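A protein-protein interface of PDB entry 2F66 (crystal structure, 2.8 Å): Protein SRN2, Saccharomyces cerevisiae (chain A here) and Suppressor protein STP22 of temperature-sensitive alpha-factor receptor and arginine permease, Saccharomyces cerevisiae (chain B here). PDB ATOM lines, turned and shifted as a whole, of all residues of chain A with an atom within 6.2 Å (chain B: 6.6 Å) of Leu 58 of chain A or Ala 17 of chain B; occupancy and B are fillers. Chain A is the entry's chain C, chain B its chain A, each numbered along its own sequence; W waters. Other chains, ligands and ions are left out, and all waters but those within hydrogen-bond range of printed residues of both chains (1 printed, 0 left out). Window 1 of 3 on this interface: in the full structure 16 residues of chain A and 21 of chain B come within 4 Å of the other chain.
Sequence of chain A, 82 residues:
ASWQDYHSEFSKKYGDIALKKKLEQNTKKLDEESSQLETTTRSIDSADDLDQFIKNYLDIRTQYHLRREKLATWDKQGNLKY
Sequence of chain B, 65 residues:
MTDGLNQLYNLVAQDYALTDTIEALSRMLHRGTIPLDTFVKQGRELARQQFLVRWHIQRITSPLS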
ATOM      1  N   PHE A  53       5.827  14.738 -17.844  1.00  0.00           N
ATOM      2  CA  PHE A  53       5.890  13.459 -17.164  1.00  0.00           C
ATOM      3  C   PHE A  53       5.812  13.634 -15.664  1.00  0.00           C
ATOM      4  O   PHE A  53       4.974  13.017 -14.993  1.00  0.00           O
ATOM      5  CB  PHE A  53       7.180  12.717 -17.494  1.00  0.00           C
ATOM      6  CG  PHE A  53       7.329  11.424 -16.741  1.00  0.00           C
ATOM      7  CD1 PHE A  53       6.517  10.334 -17.042  1.00  0.00           C
ATOM      8  CD2 PHE A  53       8.236  11.316 -15.689  1.00  0.00           C
ATOM      9  CE1 PHE A  53       6.599   9.162 -16.306  1.00  0.00           C
ATOM     10  CE2 PHE A  53       8.325  10.145 -14.946  1.00  0.00           C
ATOM     11  CZ  PHE A  53       7.503   9.063 -15.253  1.00  0.00           C
ATOM     12  N   ILE A  54       6.695  14.479 -15.139  1.00  0.00           N
ATOM     13  CA  ILE A  54       6.727  14.701 -13.711  1.00  0.00           C
ATOM     14  C   ILE A  54       5.367  15.129 -13.193  1.00  0.00           C
ATOM     15  O   ILE A  54       4.860  14.550 -12.236  1.00  0.00           O
ATOM     16  CB  ILE A  54       7.811  15.733 -13.326  1.00  0.00           C
ATOM     17  CG1 ILE A  54       9.192  15.153 -13.639  1.00  0.00           C
ATOM     18  CG2 ILE A  54       7.742  16.048 -11.840  1.00  0.00           C
ATOM     19  CD1 ILE A  54      10.355  16.010 -13.153  1.00  0.00           C
ATOM     20  N   LYS A  55       4.759  16.117 -13.839  1.00  0.00           N
ATOM     21  CA  LYS A  55       3.456  16.600 -13.400  1.00  0.00           C
ATOM     22  C   LYS A  55       2.370  15.536 -13.436  1.00  0.00           C
ATOM     23  O   LYS A  55       1.584  15.413 -12.491  1.00  0.00           O
ATOM     24  CB  LYS A  55       3.024  17.830 -14.216  1.00  0.00           C
ATOM     25  CG  LYS A  55       3.826  19.096 -13.876  1.00  0.00           C
ATOM     26  CD  LYS A  55       4.196  19.132 -12.374  1.00  0.00           C
ATOM     27  CE  LYS A  55       4.842  20.447 -11.930  1.00  0.00           C
ATOM     28  NZ  LYS A  55       3.849  21.558 -11.788  1.00  0.00           N
ATOM     29  N   ASN A  56       2.332  14.753 -14.507  1.00  0.00           N
ATOM     30  CA  ASN A  56       1.319  13.715 -14.616  1.00  0.00           C
ATOM     31  C   ASN A  56       1.586  12.539 -13.689  1.00  0.00           C
ATOM     32  O   ASN A  56       0.653  12.030 -13.070  1.00  0.00           O
ATOM     33  CB  ASN A  56       1.199  13.242 -16.064  1.00  0.00           C
ATOM     34  CG  ASN A  56       0.750  14.353 -16.995  1.00  0.00           C
ATOM     35  OD1 ASN A  56      -0.260  15.008 -16.749  1.00  0.00           O
ATOM     36  ND2 ASN A  56       1.500  14.572 -18.062  1.00  0.00           N
ATOM     37  N   TYR A  57       2.847  12.116 -13.579  1.00  0.00           N
ATOM     38  CA  TYR A  57       3.189  10.997 -12.703  1.00  0.00           C
ATOM     39  C   TYR A  57       2.879  11.358 -11.258  1.00  0.00           C
ATOM     40  O   TYR A  57       2.291  10.572 -10.510  1.00  0.00           O
ATOM     41  CB  TYR A  57       4.674  10.639 -12.802  1.00  0.00           C
ATOM     42  CG  TYR A  57       4.991   9.305 -12.147  1.00  0.00           C
ATOM     43  CD1 TYR A  57       4.671   8.103 -12.784  1.00  0.00           C
ATOM     44  CD2 TYR A  57       5.530   9.243 -10.865  1.00  0.00           C
ATOM     45  CE1 TYR A  57       4.873   6.874 -12.157  1.00  0.00           C
ATOM     46  CE2 TYR A  57       5.733   8.013 -10.222  1.00  0.00           C
ATOM     47  CZ  TYR A  57       5.398   6.835 -10.873  1.00  0.00           C
ATOM     48  OH  TYR A  57       5.549   5.623 -10.234  1.00  0.00           O
ATOM     49  N   LEU A  58       3.287  12.562 -10.879  1.00  0.00           N
ATOM     50  CA  LEU A  58       3.081  13.062  -9.531  1.00  0.00           C
ATOM     51  C   LEU A  58       1.603  13.132  -9.219  1.00  0.00           C
ATOM     52  O   LEU A  58       1.176  12.853  -8.104  1.00  0.00           O
ATOM     53  CB  LEU A  58       3.701  14.449  -9.397  1.00  0.00           C
ATOM     54  CG  LEU A  58       3.600  15.099  -8.022  1.00  0.00           C
ATOM     55  CD1 LEU A  58       4.404  14.305  -6.995  1.00  0.00           C
ATOM     56  CD2 LEU A  58       4.112  16.521  -8.127  1.00  0.00           C
ATOM     57  N   ASP A  59       0.823  13.506 -10.219  1.00  0.00           N
ATOM     58  CA  ASP A  59      -0.616  13.607 -10.051  1.00  0.00           C
ATOM     59  C   ASP A  59      -1.224  12.225  -9.805  1.00  0.00           C
ATOM     60  O   ASP A  59      -1.807  11.960  -8.753  1.00  0.00           O
ATOM     61  CB  ASP A  59      -1.232  14.229 -11.302  1.00  0.00           C
ATOM     62  CG  ASP A  59      -2.341  15.204 -10.978  1.00  0.00           C
ATOM     63  OD1 ASP A  59      -3.334  14.784 -10.342  1.00  0.00           O
ATOM     64  OD2 ASP A  59      -2.212  16.391 -11.359  1.00  0.00           O
ATOM     65  N   ILE A  60      -1.084  11.347 -10.791  1.00  0.00           N
ATOM     66  CA  ILE A  60      -1.617  10.005 -10.694  1.00  0.00           C
ATOM     67  C   ILE A  60      -1.242   9.407  -9.359  1.00  0.00           C
ATOM     68  O   ILE A  60      -2.067   8.801  -8.668  1.00  0.00           O
ATOM     69  CB  ILE A  60      -1.041   9.106 -11.800  1.00  0.00           C
ATOM     70  CG1 ILE A  60      -1.448   9.654 -13.169  1.00  0.00           C
ATOM     71  CG2 ILE A  60      -1.523   7.666 -11.608  1.00  0.00           C
ATOM     72  CD1 ILE A  60      -0.636   9.094 -14.307  1.00  0.00           C
ATOM     73  N   ARG A  61       0.018   9.598  -9.007  1.00  0.00           N
ATOM     74  CA  ARG A  61       0.570   9.066  -7.778  1.00  0.00           C
ATOM     75  C   ARG A  61      -0.081   9.636  -6.515  1.00  0.00           C
ATOM     76  O   ARG A  61      -0.300   8.906  -5.545  1.00  0.00           O
ATOM     77  CB  ARG A  61       2.077   9.309  -7.786  1.00  0.00           C
ATOM     78  CG  ARG A  61       2.908   8.105  -7.397  1.00  0.00           C
ATOM     79  CD  ARG A  61       2.499   6.851  -8.126  1.00  0.00           C
ATOM     80  NE  ARG A  61       2.603   5.733  -7.191  1.00  0.00           N
ATOM     81  CZ  ARG A  61       2.035   4.542  -7.352  1.00  0.00           C
ATOM     82  NH1 ARG A  61       1.302   4.279  -8.428  1.00  0.00           N
ATOM     83  NH2 ARG A  61       2.190   3.618  -6.421  1.00  0.00           N
ATOM     84  N   THR A  62      -0.397  10.930  -6.527  1.00  0.00           N
ATOM     85  CA  THR A  62      -1.039  11.566  -5.375  1.00  0.00           C
ATOM     86  C   THR A  62      -2.444  11.018  -5.210  1.00  0.00           C
ATOM     87  O   THR A  62      -2.809  10.540  -4.132  1.00  0.00           O
ATOM     88  CB  THR A  62      -1.171  13.088  -5.538  1.00  0.00           C
ATOM     89  OG1 THR A  62       0.118  13.671  -5.747  1.00  0.00           O
ATOM     90  CG2 THR A  62      -1.778  13.689  -4.291  1.00  0.00           C
ATOM     91  N   GLN A  63      -3.231  11.109  -6.284  1.00  0.00           N
ATOM     92  CA  GLN A  63      -4.607  10.611  -6.287  1.00  0.00           C
ATOM     93  C   GLN A  63      -4.618   9.152  -5.885  1.00  0.00           C
ATOM     94  O   GLN A  63      -5.537   8.690  -5.218  1.00  0.00           O
ATOM     95  CB  GLN A  63      -5.246  10.772  -7.668  1.00  0.00           C
ATOM     96  CG  GLN A  63      -5.621  12.220  -8.011  1.00  0.00           C
ATOM     97  CD  GLN A  63      -6.644  12.825  -7.040  1.00  0.00           C
ATOM     98  OE1 GLN A  63      -7.806  12.409  -6.994  1.00  0.00           O
ATOM     99  NE2 GLN A  63      -6.208  13.810  -6.261  1.00  0.00           N
ATOM    100  N   HIS A  65      -2.451   7.584  -3.796  1.00  0.00           N
ATOM    101  CA  HIS A  65      -2.290   7.501  -2.352  1.00  0.00           C
ATOM    102  C   HIS A  65      -3.481   8.066  -1.605  1.00  0.00           C
ATOM    103  O   HIS A  65      -3.846   7.559  -0.550  1.00  0.00           O
ATOM    104  CB  HIS A  65      -1.019   8.223  -1.910  1.00  0.00           C
ATOM    105  CG  HIS A  65       0.235   7.487  -2.253  1.00  0.00           C
ATOM    106  ND1 HIS A  65       0.582   6.298  -1.652  1.00  0.00           N
ATOM    107  CD2 HIS A  65       1.201   7.746  -3.167  1.00  0.00           C
ATOM    108  CE1 HIS A  65       1.709   5.853  -2.182  1.00  0.00           C
ATOM    109  NE2 HIS A  65       2.104   6.713  -3.103  1.00  0.00           N
ATOM    110  N   VAL B  12      -0.532  14.318   3.095  1.00  0.00           N
ATOM    111  CA  VAL B  12       0.078  13.004   3.239  1.00  0.00           C
ATOM    112  C   VAL B  12       0.221  12.353   1.862  1.00  0.00           C
ATOM    113  O   VAL B  12       1.276  11.810   1.527  1.00  0.00           O
ATOM    114  CB  VAL B  12      -0.777  12.094   4.165  1.00  0.00           C
ATOM    115  CG1 VAL B  12      -0.340  10.641   4.039  1.00  0.00           C
ATOM    116  CG2 VAL B  12      -0.637  12.565   5.617  1.00  0.00           C
ATOM    117  N   ALA B  13      -0.843  12.425   1.066  1.00  0.00           N
ATOM    118  CA  ALA B  13      -0.854  11.849  -0.270  1.00  0.00           C
ATOM    119  C   ALA B  13       0.293  12.414  -1.096  1.00  0.00           C
ATOM    120  O   ALA B  13       1.000  11.670  -1.791  1.00  0.00           O
ATOM    121  CB  ALA B  13      -2.174  12.143  -0.936  1.00  0.00           C
ATOM    122  N   GLN B  14       0.466  13.732  -1.011  1.00  0.00           N
ATOM    123  CA  GLN B  14       1.529  14.448  -1.722  1.00  0.00           C
ATOM    124  C   GLN B  14       2.941  14.044  -1.288  1.00  0.00           C
ATOM    125  O   GLN B  14       3.857  14.003  -2.102  1.00  0.00           O
ATOM    126  CB  GLN B  14       1.370  15.939  -1.504  1.00  0.00           C
ATOM    127  CG  GLN B  14       0.267  16.560  -2.305  1.00  0.00           C
ATOM    128  CD  GLN B  14      -0.063  17.961  -1.845  1.00  0.00           C
ATOM    129  OE1 GLN B  14       0.828  18.783  -1.613  1.00  0.00           O
ATOM    130  NE2 GLN B  14      -1.353  18.244  -1.712  1.00  0.00           N
ATOM    131  N   ASP B  15       3.114  13.775   0.002  1.00  0.00           N
ATOM    132  CA  ASP B  15       4.403  13.371   0.537  1.00  0.00           C
ATOM    133  C   ASP B  15       4.824  12.067  -0.130  1.00  0.00           C
ATOM    134  O   ASP B  15       5.904  11.984  -0.720  1.00  0.00           O
ATOM    135  CB  ASP B  15       4.304  13.185   2.064  1.00  0.00           C
ATOM    136  CG  ASP B  15       5.618  12.698   2.707  1.00  0.00           C
ATOM    137  OD1 ASP B  15       6.613  12.439   1.988  1.00  0.00           O
ATOM    138  OD2 ASP B  15       5.645  12.565   3.954  1.00  0.00           O
ATOM    139  N   TYR B  16       3.967  11.053  -0.050  1.00  0.00           N
ATOM    140  CA  TYR B  16       4.294   9.762  -0.635  1.00  0.00           C
ATOM    141  C   TYR B  16       4.446   9.828  -2.143  1.00  0.00           C
ATOM    142  O   TYR B  16       5.334   9.186  -2.706  1.00  0.00           O
ATOM    143  CB  TYR B  16       3.253   8.718  -0.231  1.00  0.00           C
ATOM    144  CG  TYR B  16       3.382   8.349   1.224  1.00  0.00           C
ATOM    145  CD1 TYR B  16       3.014   9.251   2.227  1.00  0.00           C
ATOM    146  CD2 TYR B  16       3.973   7.147   1.605  1.00  0.00           C
ATOM    147  CE1 TYR B  16       3.243   8.969   3.577  1.00  0.00           C
ATOM    148  CE2 TYR B  16       4.209   6.855   2.950  1.00  0.00           C
ATOM    149  CZ  TYR B  16       3.848   7.772   3.933  1.00  0.00           C
ATOM    150  OH  TYR B  16       4.132   7.508   5.260  1.00  0.00           O
ATOM    151  N   ALA B  17       3.593  10.611  -2.793  1.00  0.00           N
ATOM    152  CA  ALA B  17       3.671  10.757  -4.237  1.00  0.00           C
ATOM    153  C   ALA B  17       5.031  11.354  -4.596  1.00  0.00           C
ATOM    154  O   ALA B  17       5.724  10.863  -5.491  1.00  0.00           O
ATOM    155  CB  ALA B  17       2.554  11.656  -4.732  1.00  0.00           C
ATOM    156  N   LEU B  18       5.418  12.408  -3.886  1.00  0.00           N
ATOM    157  CA  LEU B  18       6.700  13.058  -4.130  1.00  0.00           C
ATOM    158  C   LEU B  18       7.864  12.072  -4.078  1.00  0.00           C
ATOM    159  O   LEU B  18       8.823  12.187  -4.851  1.00  0.00           O
ATOM    160  CB  LEU B  18       6.921  14.191  -3.125  1.00  0.00           C
ATOM    161  CG  LEU B  18       6.174  15.483  -3.483  1.00  0.00           C
ATOM    162  CD1 LEU B  18       6.272  16.497  -2.341  1.00  0.00           C
ATOM    163  CD2 LEU B  18       6.758  16.056  -4.774  1.00  0.00           C
ATOM    164  N   THR B  19       7.788  11.103  -3.171  1.00  0.00           N
ATOM    165  CA  THR B  19       8.849  10.117  -3.068  1.00  0.00           C
ATOM    166  C   THR B  19       8.818   9.227  -4.298  1.00  0.00           C
ATOM    167  O   THR B  19       9.853   8.980  -4.926  1.00  0.00           O
ATOM    168  CB  THR B  19       8.698   9.262  -1.808  1.00  0.00           C
ATOM    169  OG1 THR B  19       9.021  10.056  -0.661  1.00  0.00           O
ATOM    170  CG2 THR B  19       9.623   8.060  -1.862  1.00  0.00           C
ATOM    171  N   ASP B  20       7.617   8.767  -4.646  1.00  0.00           N
ATOM    172  CA  ASP B  20       7.422   7.909  -5.809  1.00  0.00           C
ATOM    173  C   ASP B  20       7.965   8.555  -7.082  1.00  0.00           C
ATOM    174  O   ASP B  20       8.610   7.904  -7.911  1.00  0.00           O
ATOM    175  CB  ASP B  20       5.936   7.616  -6.017  1.00  0.00           C
ATOM    176  CG  ASP B  20       5.342   6.819  -4.895  1.00  0.00           C
ATOM    177  OD1 ASP B  20       6.107   6.110  -4.206  1.00  0.00           O
ATOM    178  OD2 ASP B  20       4.106   6.887  -4.716  1.00  0.00           O
ATOM    179  N   THR B  21       7.691   9.838  -7.240  1.00  0.00           N
ATOM    180  CA  THR B  21       8.143  10.541  -8.420  1.00  0.00           C
ATOM    181  C   THR B  21       9.655  10.646  -8.457  1.00  0.00           C
ATOM    182  O   THR B  21      10.268  10.554  -9.528  1.00  0.00           O
ATOM    183  CB  THR B  21       7.512  11.918  -8.474  1.00  0.00           C
ATOM    184  OG1 THR B  21       6.088  11.766  -8.443  1.00  0.00           O
ATOM    185  CG2 THR B  21       7.911  12.640  -9.739  1.00  0.00           C
ATOM    186  N   ILE B  22      10.264  10.832  -7.291  1.00  0.00           N
ATOM    187  CA  ILE B  22      11.717  10.918  -7.236  1.00  0.00           C
ATOM    188  C   ILE B  22      12.266   9.561  -7.678  1.00  0.00           C
ATOM    189  O   ILE B  22      13.065   9.483  -8.615  1.00  0.00           O
ATOM    190  CB  ILE B  22      12.195  11.285  -5.821  1.00  0.00           C
ATOM    191  CG1 ILE B  22      11.747  12.717  -5.506  1.00  0.00           C
ATOM    192  CG2 ILE B  22      13.706  11.164  -5.726  1.00  0.00           C
ATOM    193  CD1 ILE B  22      12.036  13.190  -4.099  1.00  0.00           C
ATOM    194  N   LEU B  46      11.699  18.432  -6.270  1.00  0.00           N
ATOM    195  CA  LEU B  46      10.643  17.601  -5.700  1.00  0.00           C
ATOM    196  C   LEU B  46      10.894  17.350  -4.220  1.00  0.00           C
ATOM    197  O   LEU B  46       9.968  17.341  -3.403  1.00  0.00           O
ATOM    198  CB  LEU B  46      10.564  16.267  -6.445  1.00  0.00           C
ATOM    199  CG  LEU B  46      10.156  16.307  -7.927  1.00  0.00           C
ATOM    200  CD1 LEU B  46      10.328  14.930  -8.542  1.00  0.00           C
ATOM    201  CD2 LEU B  46       8.715  16.767  -8.055  1.00  0.00           C
ATOM    202  N   GLN B  49      10.142  20.434  -2.246  1.00  0.00           N
ATOM    203  CA  GLN B  49       8.695  20.515  -2.119  1.00  0.00           C
ATOM    204  C   GLN B  49       8.221  19.553  -1.038  1.00  0.00           C
ATOM    205  O   GLN B  49       7.326  19.868  -0.270  1.00  0.00           O
ATOM    206  CB  GLN B  49       8.013  20.168  -3.444  1.00  0.00           C
ATOM    207  CG  GLN B  49       8.025  21.286  -4.462  1.00  0.00           C
ATOM    208  CD  GLN B  49       7.308  20.907  -5.750  1.00  0.00           C
ATOM    209  OE1 GLN B  49       6.141  20.493  -5.730  1.00  0.00           O
ATOM    210  NE2 GLN B  49       8.003  21.047  -6.880  1.00  0.00           N
ATOM    211  N   GLN B  50       8.839  18.382  -0.978  1.00  0.00           N
ATOM    212  CA  GLN B  50       8.453  17.391   0.010  1.00  0.00           C
ATOM    213  C   GLN B  50       8.640  17.880   1.435  1.00  0.00           C
ATOM    214  O   GLN B  50       7.768  17.691   2.281  1.00  0.00           O
ATOM    215  CB  GLN B  50       9.242  16.105  -0.182  1.00  0.00           C
ATOM    216  CG  GLN B  50       8.740  14.975   0.695  1.00  0.00           C
ATOM    217  CD  GLN B  50       9.455  13.683   0.419  1.00  0.00           C
ATOM    218  OE1 GLN B  50      10.658  13.569   0.647  1.00  0.00           O
ATOM    219  NE2 GLN B  50       8.721  12.696  -0.087  1.00  0.00           N
HETATM  220  O   HOH W   1       7.597   5.215  -8.393  1.00  0.00           O
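The side-chain carboxylate of Asp 20 of chain B sits at hydrogen-bond distance from a ring nitrogen (NE2) of His 65 of chain A, 2.6 Å away. OD2 of Asp 20 of chain B lies within salt-bridge range of NE of Arg 61 of chain A (3.1 Å).
O of Leu 58 of chain A is in hydrogen-bond range of OG1 of Thr 62 of chain A (2.7 Å). O of Ala 17 of chain B is in hydrogen-bond range of OG1 of Thr 21 of chain B, at 3.1 Å.
Among the printed residues, merely in contact across the chains: Thr 62 of chain A with Ala 17 of chain B, Leu 58 of chain A with Thr 21 of chain B, Tyr 57 of chain A with Thr 21 of chain B, Thr 62 of chain A with Ala 13 of chain B, Leu 58 of chain A with Leu 18 of chain B, His 65 of chain A with Tyr 16 of chain B, Tyr 57 of chain A with Asp 20 of chain B, His 65 of chain A with Ala 17 of chain B, Arg 61 of chain A with Ala 17 of chain B, Leu 58 of chain A with Ala 17 of chain B, Ile 54 of chain A with Leu 46 of chain B, Thr 62 of chain A with Gln 14 of chain B and His 65 of chain A with Ala 13 of chain B.
Of the printed residues of chain B, Leu 58 of chain A touches Ala 17, Leu 18 and Thr 21. Printed residues of chain A within 4 Å of Tyr 16 of chain B: His 65 (3.7 Å). Printed residues of chain A within 4 Å of Thr 21 of chain B: Tyr 57 and Leu 58. Printed residues of chain B within 4 Å of Tyr 57 of chain A: Asp 20 and Thr 21. Of the printed residues of chain B, Arg 61 of chain A touches Ala 17 (3.8 Å) and Asp 20 (3.1 Å). Of the printed residues of chain A, Gln 14 of chain B touches Thr 62. Gln 49 of chain B touches none of the printed residues of chain A. The nearest residue of chain B that does not touch Leu 58 of chain A is Leu 46 of chain B (4.6 Å). The nearest printed residue of chain A that does not touch Leu 46 of chain B is Leu 58 of chain A (4.6 Å).
Of the 12 printed residues of chain A, 6 touch a printed residue of chain B. Hydrophobic or aromatic side chains of chain A within 4 Å of the printed part of chain B: Ile 54, Tyr 57, Leu 58 and His 65. Among the printed residues, 15 pairs touch across the chains.
Water W1 bridges the side-chain hydroxyl of Tyr 57 of chain A (2.8 Å) and the backbone carbonyl oxygen of Asp 20 of chain B (2.9 Å).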
